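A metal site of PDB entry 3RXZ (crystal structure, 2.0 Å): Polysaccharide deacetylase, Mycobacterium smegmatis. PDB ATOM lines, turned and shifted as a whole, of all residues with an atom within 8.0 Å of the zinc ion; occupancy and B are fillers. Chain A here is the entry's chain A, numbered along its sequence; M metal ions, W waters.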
ATOM      1  N   PHE A  31     -25.189  11.895  17.053  1.00  0.00           N
ATOM      2  CA  PHE A  31     -23.823  11.642  17.549  1.00  0.00           C
ATOM      3  C   PHE A  31     -22.878  12.273  16.638  1.00  0.00           C
ATOM      4  O   PHE A  31     -22.980  12.050  15.427  1.00  0.00           O
ATOM      5  CB  PHE A  31     -23.497  10.092  17.614  1.00  0.00           C
ATOM      6  CG  PHE A  31     -24.511   9.304  18.382  1.00  0.00           C
ATOM      7  CD1 PHE A  31     -24.373   9.106  19.760  1.00  0.00           C
ATOM      8  CD2 PHE A  31     -25.702   8.874  17.759  1.00  0.00           C
ATOM      9  CE1 PHE A  31     -25.410   8.520  20.492  1.00  0.00           C
ATOM     10  CE2 PHE A  31     -26.699   8.207  18.485  1.00  0.00           C
ATOM     11  CZ  PHE A  31     -26.546   8.018  19.838  1.00  0.00           C
ATOM     12  N   ASP A  32     -21.983  13.085  17.184  1.00  0.00           N
ATOM     13  CA  ASP A  32     -20.921  13.749  16.435  1.00  0.00           C
ATOM     14  C   ASP A  32     -19.667  12.945  16.692  1.00  0.00           C
ATOM     15  O   ASP A  32     -19.167  12.912  17.828  1.00  0.00           O
ATOM     16  CB  ASP A  32     -20.775  15.228  16.862  1.00  0.00           C
ATOM     17  CG  ASP A  32     -22.003  16.156  16.641  1.00  0.00           C
ATOM     18  OD1 ASP A  32     -22.928  15.760  15.903  1.00  0.00           O
ATOM     19  OD2 ASP A  32     -21.998  17.284  17.174  1.00  0.00           O
ATOM     20  N   VAL A  33     -19.227  12.213  15.674  1.00  0.00           N
ATOM     21  CA  VAL A  33     -18.043  11.340  15.770  1.00  0.00           C
ATOM     22  C   VAL A  33     -16.783  12.189  15.476  1.00  0.00           C
ATOM     23  O   VAL A  33     -16.092  12.031  14.459  1.00  0.00           O
ATOM     24  CB  VAL A  33     -18.208  10.116  14.870  1.00  0.00           C
ATOM     25  CG1 VAL A  33     -17.182   9.061  15.281  1.00  0.00           C
ATOM     26  CG2 VAL A  33     -19.644   9.520  15.037  1.00  0.00           C
ATOM     27  N   ASP A  34     -16.559  13.165  16.378  1.00  0.00           N
ATOM     28  CA  ASP A  34     -15.508  14.190  16.320  1.00  0.00           C
ATOM     29  C   ASP A  34     -14.154  13.568  16.495  1.00  0.00           C
ATOM     30  O   ASP A  34     -13.221  13.918  15.763  1.00  0.00           O
ATOM     31  CB  ASP A  34     -15.745  15.257  17.370  1.00  0.00           C
ATOM     32  CG  ASP A  34     -16.972  16.142  17.073  1.00  0.00           C
ATOM     33  OD1 ASP A  34     -17.526  16.004  16.001  1.00  0.00           O
ATOM     34  OD2 ASP A  34     -17.323  16.987  17.929  1.00  0.00           O
ATOM     35  N   ALA A  35     -14.038  12.624  17.421  1.00  0.00           N
ATOM     36  CA  ALA A  35     -12.769  11.909  17.635  1.00  0.00           C
ATOM     37  C   ALA A  35     -11.618  12.921  17.784  1.00  0.00           C
ATOM     38  O   ALA A  35     -11.721  13.884  18.570  1.00  0.00           O
ATOM     39  CB  ALA A  35     -12.534  10.912  16.465  1.00  0.00           C
ATOM     40  N   SER A  37     -10.288  15.020  15.396  1.00  0.00           N
ATOM     41  CA  SER A  37     -10.436  16.231  14.549  1.00  0.00           C
ATOM     42  C   SER A  37     -10.611  17.625  15.307  1.00  0.00           C
ATOM     43  O   SER A  37      -9.925  18.539  14.882  1.00  0.00           O
ATOM     44  CB  SER A  37     -11.539  16.049  13.501  1.00  0.00           C
ATOM     45  OG  SER A  37     -12.826  15.867  14.058  1.00  0.00           O
ATOM     46  N   PRO A  38     -11.456  17.873  16.330  1.00  0.00           N
ATOM     47  CA  PRO A  38     -11.501  19.243  16.924  1.00  0.00           C
ATOM     48  C   PRO A  38     -10.155  19.704  17.524  1.00  0.00           C
ATOM     49  O   PRO A  38      -9.796  20.882  17.469  1.00  0.00           O
ATOM     50  CB  PRO A  38     -12.539  19.098  18.056  1.00  0.00           C
ATOM     51  CG  PRO A  38     -13.267  17.876  17.792  1.00  0.00           C
ATOM     52  CD  PRO A  38     -12.372  16.970  17.039  1.00  0.00           C
ATOM     53  N   PHE A  81     -23.062  12.524  12.809  1.00  0.00           N
ATOM     54  CA  PHE A  81     -22.409  13.648  12.117  1.00  0.00           C
ATOM     55  C   PHE A  81     -20.912  13.289  12.131  1.00  0.00           C
ATOM     56  O   PHE A  81     -20.278  13.177  13.194  1.00  0.00           O
ATOM     57  CB  PHE A  81     -22.756  15.010  12.777  1.00  0.00           C
ATOM     58  CG  PHE A  81     -24.192  15.411  12.561  1.00  0.00           C
ATOM     59  CD1 PHE A  81     -24.555  16.214  11.493  1.00  0.00           C
ATOM     60  CD2 PHE A  81     -25.202  14.942  13.386  1.00  0.00           C
ATOM     61  CE1 PHE A  81     -25.903  16.583  11.289  1.00  0.00           C
ATOM     62  CE2 PHE A  81     -26.534  15.286  13.171  1.00  0.00           C
ATOM     63  CZ  PHE A  81     -26.880  16.106  12.106  1.00  0.00           C
ATOM     64  N   PRO A  83     -17.093  14.133  10.759  1.00  0.00           N
ATOM     65  CA  PRO A  83     -16.086  14.914  10.022  1.00  0.00           C
ATOM     66  C   PRO A  83     -15.362  14.011   9.005  1.00  0.00           C
ATOM     67  O   PRO A  83     -15.105  12.839   9.266  1.00  0.00           O
ATOM     68  CB  PRO A  83     -15.122  15.423  11.135  1.00  0.00           C
ATOM     69  CG  PRO A  83     -16.008  15.411  12.425  1.00  0.00           C
ATOM     70  CD  PRO A  83     -16.821  14.135  12.238  1.00  0.00           C
ATOM     71  N   HIS A 107     -20.060  17.044   8.896  1.00  0.00           N
ATOM     72  CA  HIS A 107     -19.574  17.769  10.072  1.00  0.00           C
ATOM     73  C   HIS A 107     -18.140  18.296   9.771  1.00  0.00           C
ATOM     74  O   HIS A 107     -17.209  18.135  10.561  1.00  0.00           O
ATOM     75  CB  HIS A 107     -19.643  16.850  11.299  1.00  0.00           C
ATOM     76  CG  HIS A 107     -19.665  17.552  12.614  1.00  0.00           C
ATOM     77  ND1 HIS A 107     -20.346  18.755  12.788  1.00  0.00           N
ATOM     78  CD2 HIS A 107     -19.088  17.195  13.796  1.00  0.00           C
ATOM     79  CE1 HIS A 107     -20.188  19.087  14.070  1.00  0.00           C
ATOM     80  NE2 HIS A 107     -19.416  18.211  14.728  1.00  0.00           N
ATOM     81  N   HIS A 111     -13.128  19.146  11.072  1.00  0.00           N
ATOM     82  CA  HIS A 111     -13.968  19.800  12.077  1.00  0.00           C
ATOM     83  C   HIS A 111     -13.584  21.310  12.265  1.00  0.00           C
ATOM     84  O   HIS A 111     -13.481  21.762  13.391  1.00  0.00           O
ATOM     85  CB  HIS A 111     -13.760  19.019  13.403  1.00  0.00           C
ATOM     86  CG  HIS A 111     -14.776  19.249  14.467  1.00  0.00           C
ATOM     87  ND1 HIS A 111     -14.735  20.383  15.276  1.00  0.00           N
ATOM     88  CD2 HIS A 111     -15.789  18.448  14.870  1.00  0.00           C
ATOM     89  CE1 HIS A 111     -15.714  20.209  16.167  1.00  0.00           C
ATOM     90  NE2 HIS A 111     -16.404  19.088  15.912  1.00  0.00           N
ATOM     91  N   ARG A 145     -24.235  19.923  10.145  1.00  0.00           N
ATOM     92  CA  ARG A 145     -24.084  20.459  11.497  1.00  0.00           C
ATOM     93  C   ARG A 145     -22.758  21.062  11.584  1.00  0.00           C
ATOM     94  O   ARG A 145     -21.771  20.382  11.314  1.00  0.00           O
ATOM     95  CB  ARG A 145     -24.227  19.388  12.531  1.00  0.00           C
ATOM     96  CG  ARG A 145     -23.975  19.880  13.936  1.00  0.00           C
ATOM     97  CD  ARG A 145     -24.339  18.801  14.879  1.00  0.00           C
ATOM     98  NE  ARG A 145     -25.775  18.662  15.031  1.00  0.00           N
ATOM     99  CZ  ARG A 145     -26.378  17.753  15.794  1.00  0.00           C
ATOM    100  NH1 ARG A 145     -25.677  16.750  16.317  1.00  0.00           N
ATOM    101  NH2 ARG A 145     -27.686  17.765  15.928  1.00  0.00           N
ATOM    102  N   ALA A 146     -22.700  22.371  11.828  1.00  0.00           N
ATOM    103  CA  ALA A 146     -21.419  23.092  11.800  1.00  0.00           C
ATOM    104  C   ALA A 146     -20.523  22.658  12.965  1.00  0.00           C
ATOM    105  O   ALA A 146     -21.032  22.515  14.083  1.00  0.00           O
ATOM    106  CB  ALA A 146     -21.679  24.570  11.890  1.00  0.00           C
ATOM    107  N   PRO A 147     -19.218  22.378  12.731  1.00  0.00           N
ATOM    108  CA  PRO A 147     -18.341  22.081  13.864  1.00  0.00           C
ATOM    109  C   PRO A 147     -18.339  23.260  14.860  1.00  0.00           C
ATOM    110  O   PRO A 147     -18.401  24.431  14.456  1.00  0.00           O
ATOM    111  CB  PRO A 147     -16.996  21.863  13.229  1.00  0.00           C
ATOM    112  CG  PRO A 147     -17.309  21.523  11.738  1.00  0.00           C
ATOM    113  CD  PRO A 147     -18.474  22.410  11.441  1.00  0.00           C
ATOM    114  N   MET A 148     -18.368  22.949  16.187  1.00  0.00           N
ATOM    115  CA  MET A 148     -18.415  23.897  17.300  1.00  0.00           C
ATOM    116  C   MET A 148     -19.774  24.636  17.285  1.00  0.00           C
ATOM    117  O   MET A 148     -19.962  25.592  18.033  1.00  0.00           O
ATOM    118  CB  MET A 148     -17.248  24.943  17.338  1.00  0.00           C
ATOM    119  CG  MET A 148     -15.849  24.335  17.459  1.00  0.00           C
ATOM    120  SD  MET A 148     -15.159  23.914  15.708  1.00  0.00           S
ATOM    121  CE  MET A 148     -13.231  23.565  16.294  1.00  0.00           C
ATOM    122  N   TRP A 149     -20.686  24.222  16.405  1.00  0.00           N
ATOM    123  CA  TRP A 149     -22.041  24.737  16.370  1.00  0.00           C
ATOM    124  C   TRP A 149     -22.020  26.238  16.086  1.00  0.00           C
ATOM    125  O   TRP A 149     -22.813  26.994  16.661  1.00  0.00           O
ATOM    126  CB  TRP A 149     -22.765  24.403  17.708  1.00  0.00           C
ATOM    127  CG  TRP A 149     -23.572  23.148  17.615  1.00  0.00           C
ATOM    128  CD1 TRP A 149     -23.968  22.520  16.465  1.00  0.00           C
ATOM    129  CD2 TRP A 149     -24.053  22.361  18.695  1.00  0.00           C
ATOM    130  NE1 TRP A 149     -24.725  21.420  16.783  1.00  0.00           N
ATOM    131  CE2 TRP A 149     -24.742  21.262  18.136  1.00  0.00           C
ATOM    132  CE3 TRP A 149     -24.050  22.508  20.087  1.00  0.00           C
ATOM    133  CZ2 TRP A 149     -25.366  20.300  18.916  1.00  0.00           C
ATOM    134  CZ3 TRP A 149     -24.692  21.571  20.865  1.00  0.00           C
ATOM    135  CH2 TRP A 149     -25.350  20.499  20.285  1.00  0.00           C
ATOM    136  N   ASP A 196     -26.418  18.442  24.907  1.00  0.00           N
ATOM    137  CA  ASP A 196     -25.077  18.072  24.492  1.00  0.00           C
ATOM    138  C   ASP A 196     -24.411  17.368  25.694  1.00  0.00           C
ATOM    139  O   ASP A 196     -24.630  17.791  26.833  1.00  0.00           O
ATOM    140  CB  ASP A 196     -24.330  19.362  24.106  1.00  0.00           C
ATOM    141  CG  ASP A 196     -23.056  19.205  23.309  1.00  0.00           C
ATOM    142  OD1 ASP A 196     -22.658  18.045  23.039  1.00  0.00           O
ATOM    143  OD2 ASP A 196     -22.402  20.249  23.022  1.00  0.00           O
ATOM    144  N   TRP A 198     -21.080  17.138  25.873  1.00  0.00           N
ATOM    145  CA  TRP A 198     -19.753  17.774  25.961  1.00  0.00           C
ATOM    146  C   TRP A 198     -19.562  18.527  27.269  1.00  0.00           C
ATOM    147  O   TRP A 198     -18.565  18.316  27.983  1.00  0.00           O
ATOM    148  CB  TRP A 198     -19.487  18.711  24.766  1.00  0.00           C
ATOM    149  CG  TRP A 198     -18.039  19.124  24.624  1.00  0.00           C
ATOM    150  CD1 TRP A 198     -17.383  20.077  25.352  1.00  0.00           C
ATOM    151  CD2 TRP A 198     -17.093  18.614  23.659  1.00  0.00           C
ATOM    152  NE1 TRP A 198     -16.096  20.239  24.860  1.00  0.00           N
ATOM    153  CE2 TRP A 198     -15.894  19.352  23.820  1.00  0.00           C
ATOM    154  CE3 TRP A 198     -17.192  17.725  22.569  1.00  0.00           C
ATOM    155  CZ2 TRP A 198     -14.760  19.156  22.990  1.00  0.00           C
ATOM    156  CZ3 TRP A 198     -16.078  17.542  21.745  1.00  0.00           C
ATOM    157  CH2 TRP A 198     -14.888  18.236  21.958  1.00  0.00           C
ATOM    158  N   THR A 240     -27.548  15.528  21.308  1.00  0.00           N
ATOM    159  CA  THR A 240     -26.206  15.370  20.706  1.00  0.00           C
ATOM    160  C   THR A 240     -25.239  14.683  21.711  1.00  0.00           C
ATOM    161  O   THR A 240     -25.059  15.168  22.819  1.00  0.00           O
ATOM    162  CB  THR A 240     -25.611  16.711  20.229  1.00  0.00           C
ATOM    163  OG1 THR A 240     -26.536  17.365  19.344  1.00  0.00           O
ATOM    164  CG2 THR A 240     -24.241  16.516  19.509  1.00  0.00           C
ATOM    165  N   ASN A 241     -24.609  13.590  21.306  1.00  0.00           N
ATOM    166  CA  ASN A 241     -23.620  12.823  22.090  1.00  0.00           C
ATOM    167  C   ASN A 241     -22.416  12.560  21.240  1.00  0.00           C
ATOM    168  O   ASN A 241     -22.476  12.700  20.029  1.00  0.00           O
ATOM    169  CB  ASN A 241     -24.206  11.485  22.646  1.00  0.00           C
ATOM    170  CG  ASN A 241     -25.271  11.672  23.728  1.00  0.00           C
ATOM    171  OD1 ASN A 241     -25.885  10.729  24.170  1.00  0.00           O
ATOM    172  ND2 ASN A 241     -25.446  12.871  24.258  1.00  0.00           N
ATOM    173  N   HIS A 242     -21.263  12.384  21.909  1.00  0.00           N
ATOM    174  CA  HIS A 242     -19.956  12.154  21.262  1.00  0.00           C
ATOM    175  C   HIS A 242     -19.537  10.795  21.677  1.00  0.00           C
ATOM    176  O   HIS A 242     -19.416  10.582  22.884  1.00  0.00           O
ATOM    177  CB  HIS A 242     -18.892  13.215  21.668  1.00  0.00           C
ATOM    178  CG  HIS A 242     -19.352  14.625  21.309  1.00  0.00           C
ATOM    179  ND1 HIS A 242     -20.340  15.268  22.058  1.00  0.00           N
ATOM    180  CD2 HIS A 242     -19.046  15.386  20.241  1.00  0.00           C
ATOM    181  CE1 HIS A 242     -20.531  16.442  21.439  1.00  0.00           C
ATOM    182  NE2 HIS A 242     -19.727  16.563  20.370  1.00  0.00           N
ATOM    183  N   PHE A 244     -16.677   9.439  22.000  1.00  0.00           N
ATOM    184  CA  PHE A 244     -15.458   9.425  22.849  1.00  0.00           C
ATOM    185  C   PHE A 244     -15.802   9.767  24.285  1.00  0.00           C
ATOM    186  O   PHE A 244     -15.045   9.382  25.173  1.00  0.00           O
ATOM    187  CB  PHE A 244     -14.267  10.283  22.304  1.00  0.00           C
ATOM    188  CG  PHE A 244     -14.462  11.781  22.510  1.00  0.00           C
ATOM    189  CD1 PHE A 244     -15.234  12.537  21.628  1.00  0.00           C
ATOM    190  CD2 PHE A 244     -13.869  12.430  23.597  1.00  0.00           C
ATOM    191  CE1 PHE A 244     -15.406  13.925  21.831  1.00  0.00           C
ATOM    192  CE2 PHE A 244     -14.093  13.804  23.827  1.00  0.00           C
ATOM    193  CZ  PHE A 244     -14.850  14.536  22.933  1.00  0.00           C
HETATM  194 ZN    ZN M   1     -18.377  18.346  16.686  1.00  0.00          ZN
HETATM  195  O   HOH W   1     -19.890  17.999  18.080  1.00  0.00           O
HETATM  196  O   HOH W   2     -19.073  20.468  17.440  1.00  0.00           O
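Water W1 lies within hydrogen-bond range of the side-chain carboxylate (OD2) of Asp 32 (2.4 Å) and a ring nitrogen (NE2) of His 242 (2.7 Å).
Water W1 is bound to the zinc ion (2.1 Å). The zinc ion is bound by the side-chain carboxylate (OD2) of Asp 34 (2.1 Å). The zinc ion is bound by a ring nitrogen (NE2) of His 107. NE2 of His 111 binds the zinc ion, at 2.2 Å. Water W2 is bound to the zinc ion (2.4 Å). OD1 of Asp 34 is bound to the zinc ion (2.6 Å). The zinc ion has six donor atoms within binding distance.
The backbone carbonyl oxygen (O) of Asn 241 lies within hydrogen-bond range of the backbone NH (N) of Asp 32, at 2.9 Å. OD1 of Asp 32 lies within salt-bridge range of NH1 of Arg 145 (3.0 Å). The backbone carbonyl oxygen (O) of Arg 145 sits at hydrogen-bond distance from a ring nitrogen (ND1) of His 107. The side-chain carboxylate (OD2) of Asp 34 sits close to a ring nitrogen (NE2) of His 242 (3.5 Å). A ring nitrogen (ND1) of His 111 sits at hydrogen-bond distance from the side-chain sulfur of Met 148, 3.6 Å away. The side-chain hydroxyl of Ser 37 sits at hydrogen-bond distance from the backbone carbonyl oxygen of Asp 34, at 2.6 Å.
Merely in contact with the zinc ion: Asp 32. Of the 22 residues printed, 4 come within 4 Å of the zinc ion.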
